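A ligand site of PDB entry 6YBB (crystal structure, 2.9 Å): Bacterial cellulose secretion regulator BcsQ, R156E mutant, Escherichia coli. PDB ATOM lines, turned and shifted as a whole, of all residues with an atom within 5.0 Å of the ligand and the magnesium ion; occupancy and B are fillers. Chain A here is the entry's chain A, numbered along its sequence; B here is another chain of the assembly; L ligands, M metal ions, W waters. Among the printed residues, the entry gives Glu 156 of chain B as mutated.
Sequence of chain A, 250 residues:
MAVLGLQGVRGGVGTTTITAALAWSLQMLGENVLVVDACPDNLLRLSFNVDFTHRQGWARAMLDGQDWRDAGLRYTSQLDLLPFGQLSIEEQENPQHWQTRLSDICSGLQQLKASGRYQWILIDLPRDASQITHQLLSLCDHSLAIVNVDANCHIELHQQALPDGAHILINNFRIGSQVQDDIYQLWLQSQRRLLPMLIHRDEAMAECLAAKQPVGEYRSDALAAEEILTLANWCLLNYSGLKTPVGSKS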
ATOM      1  N   ARG A  10     -30.539 -18.644 -19.292  1.00  0.00           N
ATOM      2  CA  ARG A  10     -29.241 -19.251 -19.016  1.00  0.00           C
ATOM      3  C   ARG A  10     -28.426 -19.191 -20.300  1.00  0.00           C
ATOM      4  O   ARG A  10     -28.981 -19.076 -21.392  1.00  0.00           O
ATOM      5  CB  ARG A  10     -29.422 -20.685 -18.504  1.00  0.00           C
ATOM      6  CG  ARG A  10     -28.152 -21.435 -18.143  1.00  0.00           C
ATOM      7  CD  ARG A  10     -27.927 -22.591 -19.095  1.00  0.00           C
ATOM      8  NE  ARG A  10     -29.090 -23.485 -19.151  1.00  0.00           N
ATOM      9  CZ  ARG A  10     -29.264 -24.424 -20.084  1.00  0.00           C
ATOM     10  NH1 ARG A  10     -28.365 -24.584 -21.049  1.00  0.00           N
ATOM     11  NH2 ARG A  10     -30.348 -25.189 -20.053  1.00  0.00           N
ATOM     12  N   GLY A  11     -27.107 -19.226 -20.154  1.00  0.00           N
ATOM     13  CA  GLY A  11     -26.252 -19.177 -21.320  1.00  0.00           C
ATOM     14  C   GLY A  11     -26.384 -20.422 -22.184  1.00  0.00           C
ATOM     15  O   GLY A  11     -26.620 -21.521 -21.699  1.00  0.00           O
ATOM     16  N   GLY A  12     -26.246 -20.222 -23.486  1.00  0.00           N
ATOM     17  CA  GLY A  12     -26.224 -21.342 -24.406  1.00  0.00           C
ATOM     18  C   GLY A  12     -27.554 -21.971 -24.740  1.00  0.00           C
ATOM     19  O   GLY A  12     -27.580 -23.080 -25.276  1.00  0.00           O
ATOM     20  N   VAL A  13     -28.669 -21.307 -24.434  1.00  0.00           N
ATOM     21  CA  VAL A  13     -29.980 -21.905 -24.732  1.00  0.00           C
ATOM     22  C   VAL A  13     -30.434 -21.678 -26.156  1.00  0.00           C
ATOM     23  O   VAL A  13     -31.395 -22.315 -26.597  1.00  0.00           O
ATOM     24  CB  VAL A  13     -31.070 -21.373 -23.788  1.00  0.00           C
ATOM     25  CG1 VAL A  13     -30.902 -21.974 -22.409  1.00  0.00           C
ATOM     26  CG2 VAL A  13     -31.016 -19.865 -23.727  1.00  0.00           C
ATOM     27  N   GLY A  14     -29.791 -20.763 -26.883  1.00  0.00           N
ATOM     28  CA  GLY A  14     -30.092 -20.572 -28.286  1.00  0.00           C
ATOM     29  C   GLY A  14     -30.593 -19.195 -28.656  1.00  0.00           C
ATOM     30  O   GLY A  14     -31.303 -19.029 -29.651  1.00  0.00           O
ATOM     31  N   THR A  15     -30.223 -18.174 -27.866  1.00  0.00           N
ATOM     32  CA  THR A  15     -30.752 -16.830 -28.099  1.00  0.00           C
ATOM     33  C   THR A  15     -30.234 -16.240 -29.405  1.00  0.00           C
ATOM     34  O   THR A  15     -30.988 -15.643 -30.168  1.00  0.00           O
ATOM     35  CB  THR A  15     -30.407 -15.915 -26.921  1.00  0.00           C
ATOM     36  OG1 THR A  15     -28.981 -15.728 -26.865  1.00  0.00           O
ATOM     37  CG2 THR A  15     -30.868 -16.545 -25.626  1.00  0.00           C
ATOM     38  N   THR A  16     -28.930 -16.378 -29.663  1.00  0.00           N
ATOM     39  CA  THR A  16     -28.343 -15.766 -30.856  1.00  0.00           C
ATOM     40  C   THR A  16     -28.930 -16.364 -32.129  1.00  0.00           C
ATOM     41  O   THR A  16     -29.265 -15.632 -33.072  1.00  0.00           O
ATOM     42  CB  THR A  16     -26.827 -15.918 -30.830  1.00  0.00           C
ATOM     43  OG1 THR A  16     -26.289 -15.155 -29.747  1.00  0.00           O
ATOM     44  CG2 THR A  16     -26.214 -15.438 -32.135  1.00  0.00           C
ATOM     45  N   THR A  17     -29.077 -17.689 -32.178  1.00  0.00           N
ATOM     46  CA  THR A  17     -29.648 -18.317 -33.362  1.00  0.00           C
ATOM     47  C   THR A  17     -31.130 -17.974 -33.519  1.00  0.00           C
ATOM     48  O   THR A  17     -31.632 -17.883 -34.650  1.00  0.00           O
ATOM     49  CB  THR A  17     -29.442 -19.829 -33.307  1.00  0.00           C
ATOM     50  OG1 THR A  17     -28.045 -20.118 -33.298  1.00  0.00           O
ATOM     51  CG2 THR A  17     -30.082 -20.517 -34.498  1.00  0.00           C
ATOM     52  N   ASP A  41     -19.617 -11.467 -27.004  1.00  0.00           N
ATOM     53  CA  ASP A  41     -19.175 -12.592 -27.828  1.00  0.00           C
ATOM     54  C   ASP A  41     -19.209 -12.259 -29.310  1.00  0.00           C
ATOM     55  O   ASP A  41     -18.434 -12.811 -30.092  1.00  0.00           O
ATOM     56  CB  ASP A  41     -20.032 -13.822 -27.541  1.00  0.00           C
ATOM     57  CG  ASP A  41     -20.087 -14.166 -26.061  1.00  0.00           C
ATOM     58  OD1 ASP A  41     -19.146 -13.793 -25.329  1.00  0.00           O
ATOM     59  OD2 ASP A  41     -21.059 -14.827 -25.645  1.00  0.00           O
ATOM     60  N   LEU A  43     -21.399 -12.911 -31.688  1.00  0.00           N
ATOM     61  CA  LEU A  43     -21.701 -14.095 -32.480  1.00  0.00           C
ATOM     62  C   LEU A  43     -22.821 -13.889 -33.477  1.00  0.00           C
ATOM     63  O   LEU A  43     -22.923 -14.644 -34.446  1.00  0.00           O
ATOM     64  CB  LEU A  43     -22.061 -15.271 -31.563  1.00  0.00           C
ATOM     65  CG  LEU A  43     -20.949 -15.812 -30.671  1.00  0.00           C
ATOM     66  CD1 LEU A  43     -21.509 -16.745 -29.611  1.00  0.00           C
ATOM     67  CD2 LEU A  43     -19.913 -16.523 -31.518  1.00  0.00           C
ATOM     68  N   ASP A 124     -30.057  -8.678 -29.248  1.00  0.00           N
ATOM     69  CA  ASP A 124     -29.479  -9.923 -28.741  1.00  0.00           C
ATOM     70  C   ASP A 124     -28.826  -9.629 -27.399  1.00  0.00           C
ATOM     71  O   ASP A 124     -27.716  -9.103 -27.338  1.00  0.00           O
ATOM     72  CB  ASP A 124     -28.484 -10.488 -29.740  1.00  0.00           C
ATOM     73  CG  ASP A 124     -27.905 -11.829 -29.305  1.00  0.00           C
ATOM     74  OD1 ASP A 124     -28.463 -12.432 -28.368  1.00  0.00           O
ATOM     75  OD2 ASP A 124     -26.906 -12.264 -29.908  1.00  0.00           O
ATOM     76  N   ASN A 171     -36.913 -23.503 -26.378  1.00  0.00           N
ATOM     77  CA  ASN A 171     -36.073 -23.863 -27.504  1.00  0.00           C
ATOM     78  C   ASN A 171     -35.376 -25.172 -27.198  1.00  0.00           C
ATOM     79  O   ASN A 171     -35.240 -25.578 -26.032  1.00  0.00           O
ATOM     80  CB  ASN A 171     -35.048 -22.775 -27.818  1.00  0.00           C
ATOM     81  CG  ASN A 171     -34.198 -23.106 -29.012  1.00  0.00           C
ATOM     82  OD1 ASN A 171     -34.629 -23.818 -29.919  1.00  0.00           O
ATOM     83  ND2 ASN A 171     -32.962 -22.614 -29.024  1.00  0.00           N
ATOM     84  N   ASN A 172     -34.940 -25.850 -28.255  1.00  0.00           N
ATOM     85  CA  ASN A 172     -34.231 -27.121 -28.148  1.00  0.00           C
ATOM     86  C   ASN A 172     -35.101 -28.184 -27.465  1.00  0.00           C
ATOM     87  O   ASN A 172     -34.626 -29.005 -26.683  1.00  0.00           O
ATOM     88  CB  ASN A 172     -32.906 -26.951 -27.409  1.00  0.00           C
ATOM     89  CG  ASN A 172     -31.767 -27.637 -28.112  1.00  0.00           C
ATOM     90  OD1 ASN A 172     -31.865 -28.812 -28.473  1.00  0.00           O
ATOM     91  ND2 ASN A 172     -30.684 -26.918 -28.328  1.00  0.00           N
ATOM     92  N   ILE A 199     -39.889 -24.269 -30.052  1.00  0.00           N
ATOM     93  CA  ILE A 199     -38.935 -24.540 -31.114  1.00  0.00           C
ATOM     94  C   ILE A 199     -38.285 -25.874 -30.814  1.00  0.00           C
ATOM     95  O   ILE A 199     -37.548 -26.017 -29.826  1.00  0.00           O
ATOM     96  CB  ILE A 199     -37.895 -23.424 -31.233  1.00  0.00           C
ATOM     97  CG1 ILE A 199     -38.592 -22.073 -31.390  1.00  0.00           C
ATOM     98  CG2 ILE A 199     -36.973 -23.665 -32.410  1.00  0.00           C
ATOM     99  CD1 ILE A 199     -37.654 -20.900 -31.297  1.00  0.00           C
ATOM    100  N   HIS A 200     -38.549 -26.871 -31.657  1.00  0.00           N
ATOM    101  CA  HIS A 200     -37.960 -28.187 -31.473  1.00  0.00           C
ATOM    102  C   HIS A 200     -36.458 -28.155 -31.759  1.00  0.00           C
ATOM    103  O   HIS A 200     -35.934 -27.234 -32.390  1.00  0.00           O
ATOM    104  CB  HIS A 200     -38.621 -29.224 -32.379  1.00  0.00           C
ATOM    105  CG  HIS A 200     -39.988 -29.618 -31.940  1.00  0.00           C
ATOM    106  ND1 HIS A 200     -41.122 -28.917 -32.300  1.00  0.00           N
ATOM    107  CD2 HIS A 200     -40.414 -30.641 -31.160  1.00  0.00           C
ATOM    108  CE1 HIS A 200     -42.178 -29.491 -31.768  1.00  0.00           C
ATOM    109  NE2 HIS A 200     -41.781 -30.539 -31.072  1.00  0.00           N
ATOM    110  N   ARG A 201     -35.765 -29.179 -31.274  1.00  0.00           N
ATOM    111  CA  ARG A 201     -34.395 -29.401 -31.697  1.00  0.00           C
ATOM    112  C   ARG A 201     -34.402 -29.799 -33.172  1.00  0.00           C
ATOM    113  O   ARG A 201     -35.082 -30.752 -33.551  1.00  0.00           O
ATOM    114  CB  ARG A 201     -33.730 -30.473 -30.850  1.00  0.00           C
ATOM    115  CG  ARG A 201     -32.259 -30.681 -31.182  1.00  0.00           C
ATOM    116  CD  ARG A 201     -31.579 -31.627 -30.213  1.00  0.00           C
ATOM    117  NE  ARG A 201     -30.125 -31.587 -30.371  1.00  0.00           N
ATOM    118  CZ  ARG A 201     -29.320 -30.743 -29.728  1.00  0.00           C
ATOM    119  NH1 ARG A 201     -29.829 -29.868 -28.872  1.00  0.00           N
ATOM    120  NH2 ARG A 201     -28.019 -30.769 -29.943  1.00  0.00           N
ATOM    121  N   ASP A 202     -33.674 -29.051 -33.984  1.00  0.00           N
ATOM    122  CA  ASP A 202     -33.627 -29.292 -35.420  1.00  0.00           C
ATOM    123  C   ASP A 202     -32.180 -29.236 -35.871  1.00  0.00           C
ATOM    124  O   ASP A 202     -31.469 -28.288 -35.535  1.00  0.00           O
ATOM    125  CB  ASP A 202     -34.476 -28.265 -36.177  1.00  0.00           C
ATOM    126  CG  ASP A 202     -34.878 -28.730 -37.556  1.00  0.00           C
ATOM    127  OD1 ASP A 202     -33.992 -29.152 -38.331  1.00  0.00           O
ATOM    128  OD2 ASP A 202     -36.084 -28.676 -37.870  1.00  0.00           O
ATOM    129  N   GLU A 203     -31.745 -30.241 -36.623  1.00  0.00           N
ATOM    130  CA  GLU A 203     -30.391 -30.212 -37.164  1.00  0.00           C
ATOM    131  C   GLU A 203     -30.148 -28.946 -37.979  1.00  0.00           C
ATOM    132  O   GLU A 203     -28.995 -28.496 -38.080  1.00  0.00           O
ATOM    133  CB  GLU A 203     -30.125 -31.450 -38.024  1.00  0.00           C
ATOM    134  CG  GLU A 203     -29.499 -32.582 -37.249  1.00  0.00           C
ATOM    135  CD  GLU A 203     -28.094 -32.260 -36.780  1.00  0.00           C
ATOM    136  OE1 GLU A 203     -27.260 -31.855 -37.634  1.00  0.00           O
ATOM    137  OE2 GLU A 203     -27.828 -32.387 -35.563  1.00  0.00           O
ATOM    138  N   MET A 205     -30.914 -25.995 -37.099  1.00  0.00           N
ATOM    139  CA  MET A 205     -30.444 -24.966 -36.182  1.00  0.00           C
ATOM    140  C   MET A 205     -28.965 -25.142 -35.853  1.00  0.00           C
ATOM    141  O   MET A 205     -28.265 -24.154 -35.605  1.00  0.00           O
ATOM    142  CB  MET A 205     -31.272 -24.979 -34.898  1.00  0.00           C
ATOM    143  CG  MET A 205     -32.730 -24.624 -35.114  1.00  0.00           C
ATOM    144  SD  MET A 205     -33.008 -22.844 -35.138  1.00  0.00           S
ATOM    145  CE  MET A 205     -33.043 -22.475 -33.384  1.00  0.00           C
ATOM    146  N   ALA A 206     -28.477 -26.381 -35.849  1.00  0.00           N
ATOM    147  CA  ALA A 206     -27.065 -26.625 -35.615  1.00  0.00           C
ATOM    148  C   ALA A 206     -26.235 -26.350 -36.866  1.00  0.00           C
ATOM    149  O   ALA A 206     -25.071 -25.949 -36.749  1.00  0.00           O
ATOM    150  CB  ALA A 206     -26.850 -28.065 -35.152  1.00  0.00           C
ATOM    151  N   LEU A 209     -25.742 -22.001 -38.309  1.00  0.00           N
ATOM    152  CA  LEU A 209     -24.594 -21.223 -37.827  1.00  0.00           C
ATOM    153  C   LEU A 209     -23.310 -21.672 -38.514  1.00  0.00           C
ATOM    154  O   LEU A 209     -22.456 -20.843 -38.837  1.00  0.00           O
ATOM    155  CB  LEU A 209     -24.481 -21.354 -36.305  1.00  0.00           C
ATOM    156  CG  LEU A 209     -23.352 -20.569 -35.615  1.00  0.00           C
ATOM    157  CD1 LEU A 209     -23.383 -19.081 -35.986  1.00  0.00           C
ATOM    158  CD2 LEU A 209     -23.424 -20.748 -34.113  1.00  0.00           C
ATOM    159  N   ARG B  10     -18.607 -21.651 -22.725  1.00  0.00           N
ATOM    160  CA  ARG B  10     -19.770 -20.787 -22.622  1.00  0.00           C
ATOM    161  C   ARG B  10     -20.743 -21.401 -21.619  1.00  0.00           C
ATOM    162  O   ARG B  10     -20.454 -22.431 -21.000  1.00  0.00           O
ATOM    163  CB  ARG B  10     -20.453 -20.574 -23.979  1.00  0.00           C
ATOM    164  CG  ARG B  10     -20.893 -21.854 -24.666  1.00  0.00           C
ATOM    165  CD  ARG B  10     -22.059 -21.609 -25.599  1.00  0.00           C
ATOM    166  NE  ARG B  10     -22.396 -22.807 -26.364  1.00  0.00           N
ATOM    167  CZ  ARG B  10     -23.272 -23.726 -25.964  1.00  0.00           C
ATOM    168  NH1 ARG B  10     -23.884 -23.593 -24.799  1.00  0.00           N
ATOM    169  NH2 ARG B  10     -23.517 -24.786 -26.719  1.00  0.00           N
ATOM    170  N   GLY B  11     -21.903 -20.782 -21.474  1.00  0.00           N
ATOM    171  CA  GLY B  11     -22.898 -21.288 -20.564  1.00  0.00           C
ATOM    172  C   GLY B  11     -23.615 -22.514 -21.096  1.00  0.00           C
ATOM    173  O   GLY B  11     -23.525 -22.864 -22.281  1.00  0.00           O
ATOM    174  N   ASP B 150     -20.219 -27.966 -31.094  1.00  0.00           N
ATOM    175  CA  ASP B 150     -21.139 -27.202 -31.931  1.00  0.00           C
ATOM    176  C   ASP B 150     -20.378 -26.016 -32.529  1.00  0.00           C
ATOM    177  O   ASP B 150     -19.215 -25.777 -32.205  1.00  0.00           O
ATOM    178  CB  ASP B 150     -22.368 -26.747 -31.128  1.00  0.00           C
ATOM    179  CG  ASP B 150     -22.008 -25.968 -29.876  1.00  0.00           C
ATOM    180  OD1 ASP B 150     -20.824 -25.617 -29.692  1.00  0.00           O
ATOM    181  OD2 ASP B 150     -22.926 -25.724 -29.062  1.00  0.00           O
ATOM    182  N   ALA B 151     -21.060 -25.278 -33.404  1.00  0.00           N
ATOM    183  CA  ALA B 151     -20.433 -24.135 -34.039  1.00  0.00           C
ATOM    184  C   ALA B 151     -20.165 -23.012 -33.055  1.00  0.00           C
ATOM    185  O   ALA B 151     -19.244 -22.217 -33.248  1.00  0.00           O
ATOM    186  CB  ALA B 151     -21.300 -23.630 -35.194  1.00  0.00           C
ATOM    187  N   ASN B 152     -20.963 -22.927 -31.982  1.00  0.00           N
ATOM    188  CA  ASN B 152     -20.747 -21.897 -30.967  1.00  0.00           C
ATOM    189  C   ASN B 152     -19.387 -22.073 -30.303  1.00  0.00           C
ATOM    190  O   ASN B 152     -18.565 -21.149 -30.270  1.00  0.00           O
ATOM    191  CB  ASN B 152     -21.872 -21.936 -29.932  1.00  0.00           C
ATOM    192  CG  ASN B 152     -22.147 -20.581 -29.314  1.00  0.00           C
ATOM    193  OD1 ASN B 152     -21.521 -20.178 -28.329  1.00  0.00           O
ATOM    194  ND2 ASN B 152     -23.109 -19.855 -29.886  1.00  0.00           N
ATOM    195  N   GLU B 156     -15.787 -19.815 -30.210  1.00  0.00           N
ATOM    196  CA  GLU B 156     -15.188 -19.370 -28.951  1.00  0.00           C
ATOM    197  C   GLU B 156     -13.772 -19.904 -28.801  1.00  0.00           C
ATOM    198  O   GLU B 156     -12.862 -19.157 -28.387  1.00  0.00           O
ATOM    199  CB  GLU B 156     -16.063 -19.800 -27.780  1.00  0.00           C
ATOM    200  CG  GLU B 156     -17.489 -19.282 -27.810  1.00  0.00           C
ATOM    201  CD  GLU B 156     -17.639 -17.899 -27.180  1.00  0.00           C
ATOM    202  OE1 GLU B 156     -18.788 -17.454 -26.972  1.00  0.00           O
ATOM    203  OE2 GLU B 156     -16.601 -17.266 -26.881  1.00  0.00           O
HETATM  204  P1  LIG L   1     -24.468 -17.832 -25.794  1.00  0.00           P
HETATM  205  O1  LIG L   1     -23.278 -17.938 -26.677  1.00  0.00           O
HETATM  206  O2  LIG L   1     -24.194 -18.246 -24.348  1.00  0.00           O
HETATM  207  O3  LIG L   1     -25.109 -16.422 -25.780  1.00  0.00           O
HETATM  208  P2  LIG L   1     -27.081 -18.603 -26.869  1.00  0.00           P
HETATM  209  O4  LIG L   1     -28.077 -18.874 -25.812  1.00  0.00           O
HETATM  210  O5  LIG L   1     -27.124 -17.234 -27.543  1.00  0.00           O
HETATM  211  O6  LIG L   1     -25.603 -18.823 -26.325  1.00  0.00           O
HETATM  212  P3  LIG L   1     -26.465 -19.811 -29.459  1.00  0.00           P
HETATM  213  O7  LIG L   1     -25.388 -18.794 -29.576  1.00  0.00           O
HETATM  214  O8  LIG L   1     -27.594 -19.767 -30.499  1.00  0.00           O
HETATM  215  O9  LIG L   1     -27.150 -19.694 -28.028  1.00  0.00           O
HETATM  216  O10 LIG L   1     -25.862 -21.295 -29.466  1.00  0.00           O
HETATM  217  C1  LIG L   1     -26.691 -22.470 -29.321  1.00  0.00           C
HETATM  218  C2  LIG L   1     -26.035 -23.598 -30.064  1.00  0.00           C
HETATM  219  O11 LIG L   1     -26.956 -24.699 -30.177  1.00  0.00           O
HETATM  220  C3  LIG L   1     -25.642 -23.255 -31.497  1.00  0.00           C
HETATM  221  O12 LIG L   1     -24.606 -24.087 -31.987  1.00  0.00           O
HETATM  222  C4  LIG L   1     -26.969 -23.488 -32.234  1.00  0.00           C
HETATM  223  O13 LIG L   1     -26.757 -23.720 -33.628  1.00  0.00           O
HETATM  224  C5  LIG L   1     -27.509 -24.723 -31.489  1.00  0.00           C
HETATM  225  N1  LIG L   1     -28.961 -24.757 -31.366  1.00  0.00           N
HETATM  226  C6  LIG L   1     -29.781 -23.785 -30.828  1.00  0.00           C
HETATM  227  N2  LIG L   1     -31.057 -24.080 -30.878  1.00  0.00           N
HETATM  228  C7  LIG L   1     -31.096 -25.323 -31.492  1.00  0.00           C
HETATM  229  C8  LIG L   1     -32.147 -26.191 -31.833  1.00  0.00           C
HETATM  230  N3  LIG L   1     -33.432 -25.917 -31.596  1.00  0.00           N
HETATM  231  N4  LIG L   1     -31.837 -27.360 -32.415  1.00  0.00           N
HETATM  232  C9  LIG L   1     -30.550 -27.647 -32.645  1.00  0.00           C
HETATM  233  N5  LIG L   1     -29.471 -26.906 -32.379  1.00  0.00           N
HETATM  234  C10 LIG L   1     -29.809 -25.749 -31.797  1.00  0.00           C
HETATM  235 MG    MG M   1     -25.167 -16.194 -28.376  1.00  0.00          MG
HETATM  236  O   HOH W   1     -24.387 -14.402 -27.965  1.00  0.00           O
HETATM  237  O   HOH W   2     -26.681 -14.657 -26.977  1.00  0.00           O
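CD1 of Leu 43 touches the magnesium ion, 3.9 Å away. The nearest printed residue that does not touch the magnesium ion is Thr 15 (4.1 Å).
OG1 of Thr 16 sits close to OD2 of Asp 124 (3.0 Å). NE of Arg 10 of chain B lies close to OD1 of Asn 152 of chain B (3.4 Å). The backbone NH (N) of Asn 172 lies within hydrogen-bond range of the backbone carbonyl oxygen (O) of Ile 199 (3.0 Å). The side-chain amide nitrogen (ND2) of Asn 171 is in hydrogen-bond range of the backbone carbonyl oxygen (O) of Val 13, 2.9 Å away. The side-chain amide nitrogen of Asn 172 sits close to the guanidinium group of Arg 201, at 3.1 Å. The side-chain carboxylate (OD2) of Asp 150 of chain B lies within salt-bridge range of the guanidinium group (NH2) of Arg 10 of chain B, 2.6 Å away.
The backbone NH (N) of Val 13 is in hydrogen-bond range of an oxygen (O4) of the ligand. The backbone NH of Thr 15 sits at hydrogen-bond distance from an oxygen (O4) of the ligand. O of Met 205 is in hydrogen-bond range of O13 of the ligand (2.5 Å). OD1 of Asn 171 lies within hydrogen-bond range of N3 of the ligand. An oxygen (O8) of the ligand lies within hydrogen-bond range of the side-chain hydroxyl (OG1) of Thr 17, 2.9 Å away. The side-chain hydroxyl (OG1) of Thr 15 lies within hydrogen-bond range of an oxygen (O4) of the ligand. ND2 of Asn 152 of chain B lies within hydrogen-bond range of O7 of the ligand (2.5 Å). A nitrogen (N3) of the ligand is in hydrogen-bond range of the backbone carbonyl oxygen (O) of His 200. O5 of the ligand sits close to N of Thr 16. A nitrogen (N4) of the ligand lies within hydrogen-bond range of the backbone NH (N) of Asp 202, at 2.9 Å. N of Thr 17 sits at hydrogen-bond distance from O8 of the ligand (3.1 Å). N of Gly 14 lies within hydrogen-bond range of O4 of the ligand (2.8 Å). The backbone NH (N) of Gly 12 lies within hydrogen-bond range of an oxygen (O2) of the ligand (3.0 Å).
Residues that only touch the ligand: Gly 11 of chain A (3.8 Å), Asp 41 (3.96 Å), Leu 43 (3.6 Å), Asn 172 (3.6 Å), Arg 201 (3.4 Å), Ala 206 (3.5 Å) and Asp 150 of chain B (3.6 Å). Hydrophobic or aromatic side chains that line the ligand: Val 13, Leu 43, Met 205 and Ala 206. 18 residues have an atom within 4 Å of the ligand: Gly 11 of chain A, Gly 12, Val 13, Gly 14, Thr 15, Thr 16, Thr 17, Asp 41, Leu 43, Asn 171, Asn 172, His 200, Arg 201, Asp 202, Met 205, Ala 206, Asp 150 of chain B and Asn 152 of chain B. The nearest printed residue that does not touch the ligand is Ala 151 of chain B (4.0001 Å).
The magnesium ion is bound by water W1 (2.0 Å), the side-chain hydroxyl of Thr 16 (2.1 Å), an oxygen (O5) of the ligand (2.4 Å) and water W2 (2.6 Å). Slightly farther from the magnesium ion lies O3 of the ligand (2.6 Å).
Water W2 lies within hydrogen-bond range of the side-chain hydroxyl (OG1) of Thr 15, an oxygen (O3) of the ligand and the side-chain carboxylate (OD1) of Asp 124.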
